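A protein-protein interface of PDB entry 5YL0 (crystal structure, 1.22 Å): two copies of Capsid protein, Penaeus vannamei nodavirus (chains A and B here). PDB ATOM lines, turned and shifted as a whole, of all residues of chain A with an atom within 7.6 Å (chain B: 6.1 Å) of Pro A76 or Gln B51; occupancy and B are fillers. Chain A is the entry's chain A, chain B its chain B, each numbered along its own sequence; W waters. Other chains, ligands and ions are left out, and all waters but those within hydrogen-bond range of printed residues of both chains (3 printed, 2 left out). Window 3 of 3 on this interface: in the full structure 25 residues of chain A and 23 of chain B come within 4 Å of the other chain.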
ATOM      1  N   GLN A  51     -33.853 -16.844   0.129  1.00  0.00           N
ATOM      2  CA  GLN A  51     -33.871 -17.633   1.341  1.00  0.00           C
ATOM      3  C   GLN A  51     -35.270 -17.727   1.906  1.00  0.00           C
ATOM      4  O   GLN A  51     -35.435 -17.985   3.125  1.00  0.00           O
ATOM      5  CB  GLN A  51     -32.824 -17.210   2.335  1.00  0.00           C
ATOM      6  CG  GLN A  51     -32.775 -15.830   2.757  1.00  0.00           C
ATOM      7  CD  GLN A  51     -31.471 -15.396   3.432  1.00  0.00           C
ATOM      8  OE1 GLN A  51     -30.377 -15.594   2.885  1.00  0.00           O
ATOM      9  NE2 GLN A  51     -31.592 -14.716   4.584  1.00  0.00           N
ATOM     10  N   GLY A  55     -32.655 -24.623   0.658  1.00  0.00           N
ATOM     11  CA  GLY A  55     -31.969 -24.851  -0.606  1.00  0.00           C
ATOM     12  C   GLY A  55     -31.531 -23.579  -1.280  1.00  0.00           C
ATOM     13  O   GLY A  55     -31.920 -22.467  -0.900  1.00  0.00           O
ATOM     14  N   ILE A  56     -30.675 -23.745  -2.259  1.00  0.00           N
ATOM     15  CA  ILE A  56     -30.048 -22.612  -2.976  1.00  0.00           C
ATOM     16  C   ILE A  56     -30.575 -22.488  -4.362  1.00  0.00           C
ATOM     17  O   ILE A  56     -30.657 -23.466  -5.124  1.00  0.00           O
ATOM     18  CB  ILE A  56     -28.475 -22.786  -3.004  1.00  0.00           C
ATOM     19  CG1 ILE A  56     -27.931 -22.927  -1.601  1.00  0.00           C
ATOM     20  CG2 ILE A  56     -27.842 -21.637  -3.779  1.00  0.00           C
ATOM     21  CD1 ILE A  56     -26.500 -23.409  -1.523  1.00  0.00           C
ATOM     22  N   TYR A  57     -30.911 -21.246  -4.735  1.00  0.00           N
ATOM     23  CA  TYR A  57     -31.282 -20.940  -6.140  1.00  0.00           C
ATOM     24  C   TYR A  57     -30.064 -20.996  -7.051  1.00  0.00           C
ATOM     25  O   TYR A  57     -29.147 -20.199  -6.868  1.00  0.00           O
ATOM     26  CB  TYR A  57     -31.930 -19.547  -6.166  1.00  0.00           C
ATOM     27  CG  TYR A  57     -32.483 -19.161  -7.544  1.00  0.00           C
ATOM     28  CD1 TYR A  57     -31.653 -18.694  -8.536  1.00  0.00           C
ATOM     29  CD2 TYR A  57     -33.831 -19.374  -7.865  1.00  0.00           C
ATOM     30  CE1 TYR A  57     -32.159 -18.364  -9.792  1.00  0.00           C
ATOM     31  CE2 TYR A  57     -34.327 -19.051  -9.110  1.00  0.00           C
ATOM     32  CZ  TYR A  57     -33.483 -18.557 -10.074  1.00  0.00           C
ATOM     33  OH  TYR A  57     -33.930 -18.238 -11.356  1.00  0.00           O
ATOM     34  N   ASN A  73     -25.993 -18.233  -9.250  1.00  0.00           N
ATOM     35  CA  ASN A  73     -25.850 -19.059  -8.082  1.00  0.00           C
ATOM     36  C   ASN A  73     -25.915 -18.204  -6.863  1.00  0.00           C
ATOM     37  O   ASN A  73     -24.980 -17.393  -6.624  1.00  0.00           O
ATOM     38  CB  ASN A  73     -24.541 -19.863  -8.144  1.00  0.00           C
ATOM     39  CG  ASN A  73     -24.415 -20.782  -6.901  1.00  0.00           C
ATOM     40  OD1 ASN A  73     -25.160 -20.700  -5.981  1.00  0.00           O
ATOM     41  ND2 ASN A  73     -23.436 -21.721  -6.949  1.00  0.00           N
ATOM     42  N   MET A  74     -27.009 -18.277  -6.112  1.00  0.00           N
ATOM     43  CA  MET A  74     -27.208 -17.389  -4.990  1.00  0.00           C
ATOM     44  C   MET A  74     -26.607 -17.994  -3.689  1.00  0.00           C
ATOM     45  O   MET A  74     -26.888 -17.474  -2.587  1.00  0.00           O
ATOM     46  CB  MET A  74     -28.677 -17.018  -4.856  1.00  0.00           C
ATOM     47  CG  MET A  74     -29.123 -16.300  -6.112  1.00  0.00           C
ATOM     48  SD  MET A  74     -28.107 -14.971  -6.733  1.00  0.00           S
ATOM     49  CE  MET A  74     -28.060 -13.818  -5.396  1.00  0.00           C
ATOM     50  N   ASP A  75     -25.815 -19.000  -3.747  1.00  0.00           N
ATOM     51  CA  ASP A  75     -25.113 -19.513  -2.564  1.00  0.00           C
ATOM     52  C   ASP A  75     -24.421 -18.378  -1.798  1.00  0.00           C
ATOM     53  O   ASP A  75     -23.660 -17.712  -2.384  1.00  0.00           O
ATOM     54  CB  ASP A  75     -24.037 -20.480  -3.003  1.00  0.00           C
ATOM     55  CG  ASP A  75     -23.362 -21.270  -1.872  1.00  0.00           C
ATOM     56  OD1 ASP A  75     -23.299 -20.731  -0.754  1.00  0.00           O
ATOM     57  OD2 ASP A  75     -22.871 -22.365  -2.159  1.00  0.00           O
ATOM     58  N   PRO A  76     -24.750 -18.185  -0.527  1.00  0.00           N
ATOM     59  CA  PRO A  76     -24.124 -17.057   0.175  1.00  0.00           C
ATOM     60  C   PRO A  76     -22.639 -17.170   0.343  1.00  0.00           C
ATOM     61  O   PRO A  76     -21.981 -16.141   0.586  1.00  0.00           O
ATOM     62  CB  PRO A  76     -24.828 -16.988   1.547  1.00  0.00           C
ATOM     63  CG  PRO A  76     -25.728 -18.115   1.553  1.00  0.00           C
ATOM     64  CD  PRO A  76     -25.775 -18.831   0.271  1.00  0.00           C
ATOM     65  N   THR A  77     -22.080 -18.312   0.218  1.00  0.00           N
ATOM     66  CA  THR A  77     -20.636 -18.474   0.309  1.00  0.00           C
ATOM     67  C   THR A  77     -19.921 -18.210  -0.976  1.00  0.00           C
ATOM     68  O   THR A  77     -18.686 -17.910  -0.978  1.00  0.00           O
ATOM     69  CB  THR A  77     -20.253 -19.877   0.870  1.00  0.00           C
ATOM     70  OG1 THR A  77     -20.491 -20.856  -0.119  1.00  0.00           O
ATOM     71  CG2 THR A  77     -21.025 -20.238   2.109  1.00  0.00           C
ATOM     72  N   VAL A  78     -20.613 -18.247  -2.130  1.00  0.00           N
ATOM     73  CA  VAL A  78     -19.977 -18.158  -3.412  1.00  0.00           C
ATOM     74  C   VAL A  78     -21.048 -17.708  -4.445  1.00  0.00           C
ATOM     75  O   VAL A  78     -21.634 -18.535  -5.198  1.00  0.00           O
ATOM     76  CB  VAL A  78     -19.189 -19.467  -3.745  1.00  0.00           C
ATOM     77  CG1 VAL A  78     -20.062 -20.720  -3.858  1.00  0.00           C
ATOM     78  CG2 VAL A  78     -18.406 -19.281  -4.952  1.00  0.00           C
ATOM     79  N   THR A  79     -21.348 -16.436  -4.438  1.00  0.00           N
ATOM     80  CA  THR A  79     -22.507 -15.894  -5.176  1.00  0.00           C
ATOM     81  C   THR A  79     -22.053 -15.425  -6.525  1.00  0.00           C
ATOM     82  O   THR A  79     -21.055 -14.690  -6.669  1.00  0.00           O
ATOM     83  CB  THR A  79     -23.090 -14.741  -4.424  1.00  0.00           C
ATOM     84  OG1 THR A  79     -23.279 -15.064  -3.027  1.00  0.00           O
ATOM     85  CG2 THR A  79     -24.407 -14.305  -4.977  1.00  0.00           C
ATOM     86  N   GLN B  48     -18.488 -14.426  -5.333  1.00  0.00           N
ATOM     87  CA  GLN B  48     -18.239 -13.502  -4.232  1.00  0.00           C
ATOM     88  C   GLN B  48     -18.853 -13.952  -2.985  1.00  0.00           C
ATOM     89  O   GLN B  48     -19.939 -14.555  -2.947  1.00  0.00           O
ATOM     90  CB  GLN B  48     -18.787 -12.151  -4.584  1.00  0.00           C
ATOM     91  CG  GLN B  48     -18.130 -11.488  -5.762  1.00  0.00           C
ATOM     92  CD  GLN B  48     -16.656 -11.268  -5.506  1.00  0.00           C
ATOM     93  OE1 GLN B  48     -16.267 -10.595  -4.548  1.00  0.00           O
ATOM     94  NE2 GLN B  48     -15.833 -11.861  -6.349  1.00  0.00           N
ATOM     95  N   ASN B  49     -18.185 -13.724  -1.868  1.00  0.00           N
ATOM     96  CA  ASN B  49     -18.775 -13.957  -0.549  1.00  0.00           C
ATOM     97  C   ASN B  49     -19.084 -12.583   0.056  1.00  0.00           C
ATOM     98  O   ASN B  49     -18.192 -11.873   0.680  1.00  0.00           O
ATOM     99  CB  ASN B  49     -17.807 -14.722   0.370  1.00  0.00           C
ATOM    100  CG  ASN B  49     -18.353 -14.876   1.741  1.00  0.00           C
ATOM    101  OD1 ASN B  49     -19.418 -14.501   2.042  1.00  0.00           O
ATOM    102  ND2 ASN B  49     -17.486 -15.425   2.654  1.00  0.00           N
ATOM    103  N   PHE B  50     -20.302 -12.132  -0.109  1.00  0.00           N
ATOM    104  CA  PHE B  50     -20.805 -10.892   0.413  1.00  0.00           C
ATOM    105  C   PHE B  50     -21.072 -10.875   1.934  1.00  0.00           C
ATOM    106  O   PHE B  50     -21.348  -9.780   2.452  1.00  0.00           O
ATOM    107  CB  PHE B  50     -22.006 -10.419  -0.339  1.00  0.00           C
ATOM    108  CG  PHE B  50     -21.772 -10.137  -1.826  1.00  0.00           C
ATOM    109  CD1 PHE B  50     -21.133  -8.992  -2.261  1.00  0.00           C
ATOM    110  CD2 PHE B  50     -22.280 -11.037  -2.752  1.00  0.00           C
ATOM    111  CE1 PHE B  50     -20.956  -8.794  -3.599  1.00  0.00           C
ATOM    112  CE2 PHE B  50     -22.110 -10.783  -4.066  1.00  0.00           C
ATOM    113  CZ  PHE B  50     -21.527  -9.664  -4.511  1.00  0.00           C
ATOM    114  N   GLN B  51     -20.857 -12.010   2.584  1.00  0.00           N
ATOM    115  CA  GLN B  51     -21.061 -12.069   4.020  1.00  0.00           C
ATOM    116  C   GLN B  51     -19.744 -12.395   4.710  1.00  0.00           C
ATOM    117  O   GLN B  51     -19.790 -12.868   5.858  1.00  0.00           O
ATOM    118  CB  GLN B  51     -22.099 -13.148   4.276  1.00  0.00           C
ATOM    119  CG  GLN B  51     -23.479 -12.870   3.738  1.00  0.00           C
ATOM    120  CD  GLN B  51     -24.364 -14.130   3.788  1.00  0.00           C
ATOM    121  OE1 GLN B  51     -25.491 -14.103   3.348  1.00  0.00           O
ATOM    122  NE2 GLN B  51     -23.820 -15.237   4.333  1.00  0.00           N
ATOM    123  N   SER B  52     -18.622 -12.058   4.148  1.00  0.00           N
ATOM    124  CA  SER B  52     -17.314 -12.220   4.807  1.00  0.00           C
ATOM    125  C   SER B  52     -17.091 -11.305   6.008  1.00  0.00           C
ATOM    126  O   SER B  52     -16.145 -11.591   6.817  1.00  0.00           O
ATOM    127  CB  SER B  52     -16.194 -12.050   3.785  1.00  0.00           C
ATOM    128  OG  SER B  52     -16.349 -10.872   3.064  1.00  0.00           O
ATOM    129  N   GLU B  53     -17.862 -10.266   6.112  1.00  0.00           N
ATOM    130  CA  GLU B  53     -17.867  -9.359   7.284  1.00  0.00           C
ATOM    131  C   GLU B  53     -19.239  -8.729   7.343  1.00  0.00           C
ATOM    132  O   GLU B  53     -20.131  -8.963   6.486  1.00  0.00           O
ATOM    133  CB  GLU B  53     -16.727  -8.345   7.171  1.00  0.00           C
ATOM    134  CG  GLU B  53     -16.890  -7.366   6.048  1.00  0.00           C
ATOM    135  CD  GLU B  53     -16.773  -8.003   4.670  1.00  0.00           C
ATOM    136  OE1 GLU B  53     -15.720  -8.589   4.356  1.00  0.00           O
ATOM    137  OE2 GLU B  53     -17.772  -7.893   3.898  1.00  0.00           O
ATOM    138  N   ALA B  54     -19.527  -7.993   8.428  1.00  0.00           N
ATOM    139  CA  ALA B  54     -20.828  -7.443   8.680  1.00  0.00           C
ATOM    140  C   ALA B  54     -21.206  -6.417   7.622  1.00  0.00           C
ATOM    141  O   ALA B  54     -20.339  -5.881   6.942  1.00  0.00           O
ATOM    142  CB  ALA B  54     -20.906  -6.811  10.063  1.00  0.00           C
ATOM    143  N   GLY B  55     -22.455  -6.104   7.517  1.00  0.00           N
ATOM    144  CA  GLY B  55     -23.027  -5.157   6.641  1.00  0.00           C
ATOM    145  C   GLY B  55     -23.369  -5.683   5.256  1.00  0.00           C
ATOM    146  O   GLY B  55     -22.999  -6.816   4.953  1.00  0.00           O
ATOM    147  N   PRO B  76     -29.893  -9.822   2.063  1.00  0.00           N
ATOM    148  CA  PRO B  76     -30.186 -11.227   1.986  1.00  0.00           C
ATOM    149  C   PRO B  76     -31.626 -11.573   1.905  1.00  0.00           C
ATOM    150  O   PRO B  76     -31.855 -12.724   1.540  1.00  0.00           O
ATOM    151  CB  PRO B  76     -29.621 -11.794   3.322  1.00  0.00           C
ATOM    152  CG  PRO B  76     -29.518 -10.668   4.211  1.00  0.00           C
ATOM    153  CD  PRO B  76     -29.191  -9.503   3.327  1.00  0.00           C
ATOM    154  N   LYS B 106     -17.284  -3.104   2.623  1.00  0.00           N
ATOM    155  CA  LYS B 106     -17.642  -4.257   1.778  1.00  0.00           C
ATOM    156  C   LYS B 106     -16.720  -4.244   0.575  1.00  0.00           C
ATOM    157  O   LYS B 106     -17.026  -3.538  -0.364  1.00  0.00           O
ATOM    158  CB  LYS B 106     -19.078  -4.132   1.446  1.00  0.00           C
ATOM    159  CG  LYS B 106     -20.027  -4.074   2.656  1.00  0.00           C
ATOM    160  CD  LYS B 106     -20.012  -5.236   3.594  1.00  0.00           C
ATOM    161  CE  LYS B 106     -20.449  -6.544   2.967  1.00  0.00           C
ATOM    162  NZ  LYS B 106     -20.410  -7.581   3.985  1.00  0.00           N
ATOM    163  N   GLN B 108     -15.878  -6.603  -1.615  1.00  0.00           N
ATOM    164  CA  GLN B 108     -16.125  -7.613  -2.639  1.00  0.00           C
ATOM    165  C   GLN B 108     -15.929  -6.946  -3.993  1.00  0.00           C
ATOM    166  O   GLN B 108     -15.980  -5.711  -4.161  1.00  0.00           O
ATOM    167  CB  GLN B 108     -17.521  -8.182  -2.471  1.00  0.00           C
ATOM    168  CG  GLN B 108     -17.705  -9.054  -1.240  1.00  0.00           C
ATOM    169  CD  GLN B 108     -17.889  -8.276   0.062  1.00  0.00           C
ATOM    170  OE1 GLN B 108     -18.124  -7.045   0.082  1.00  0.00           O
ATOM    171  NE2 GLN B 108     -17.760  -8.987   1.173  1.00  0.00           N
HETATM  172  O   HOH W   1     -22.503 -13.864  -0.690  1.00  0.00           O
HETATM  173  O   HOH W   2     -27.438 -14.277   1.608  1.00  0.00           O
HETATM  174  O   HOH W   3     -20.721 -16.901   3.296  1.00  0.00           O
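OE1 of Gln A51 sits close to O of Pro B76 (3.5 Å).
The backbone NH (N) of Thr A79 sits at hydrogen-bond distance from the backbone carbonyl oxygen (O) of Gln B48 (2.8 Å).
O of Pro A76 lies close to OD1 of Asn B49, 3.4 Å away.
Ile A56 touches none of the printed residues of chain B.
Pro A76 touches just these residues of chain B: Asn B49 (3.4 Å) and Gln B51 (3.4 Å).
Printed residues of chain B within 4 Å of Thr A77: Asn B49 (3.6 Å).
Printed residues of chain B within 4 Å of Val A78: Gln B48.
Of the printed residues of chain B, Thr A79 touches Gln B48 (2.8 Å).
Printed residues of chain A within 4 Å of Gln B48: Val A78 (3.6 Å) and Thr A79 (2.8 Å).
Gln B51 touches one residue of chain A.
Gly B55 touches none of the printed residues of chain A.
The nearest printed residue of chain B that does not touch Thr A79 is Phe B50 (4.1 Å).
Gln A51 touches Pro B76, and with the chains exchanged Pro A76 touches Gln B51.
Of the 6 pairs that touch across the chains among the printed residues, 2 have their exchanged pair printed and touching as well.
Among the printed residues, merely in contact across the chains: Pro A76 with Gln B51 (3.4 Å), Thr A77 with Asn B49 (3.6 Å) and Val A78 with Gln B48 (3.6 Å).
Hydrophobic or aromatic side chains of chain B within 4 Å of the printed part of chain A: Pro B76.
Among the printed residues, 6 pairs touch across the chains.
The side-chain carboxylate of Asp A75 lies within hydrogen-bond range of the backbone NH of Thr A77, 2.9 Å away.
The backbone carbonyl oxygen of Asn B49 lies within hydrogen-bond range of the side-chain amide nitrogen of Gln B108 (3.0 Å).
O of Asp A75 lies within hydrogen-bond range of OG1 of Thr A79 (2.8 Å).
OD1 of Asn B49 lies within hydrogen-bond range of N of Gln B51, at 2.9 Å.
OG of Ser B52 lies within hydrogen-bond range of O of Asn B49 (3.2 Å).
Water W2 lies within hydrogen-bond range of OE1 of Gln B51 and OE1 of Gln A51.
Water W1 lies within hydrogen-bond range of O of Pro A76 (2.7 Å), OG1 of Thr A79 (2.7 Å), N of Phe B50 (2.9 Å) and O of Gln B48 (3.5 Å).
Water W3 lies within hydrogen-bond range of OD1 of Asn B49 (3.0 Å) and O of Pro A76 (3.1 Å).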
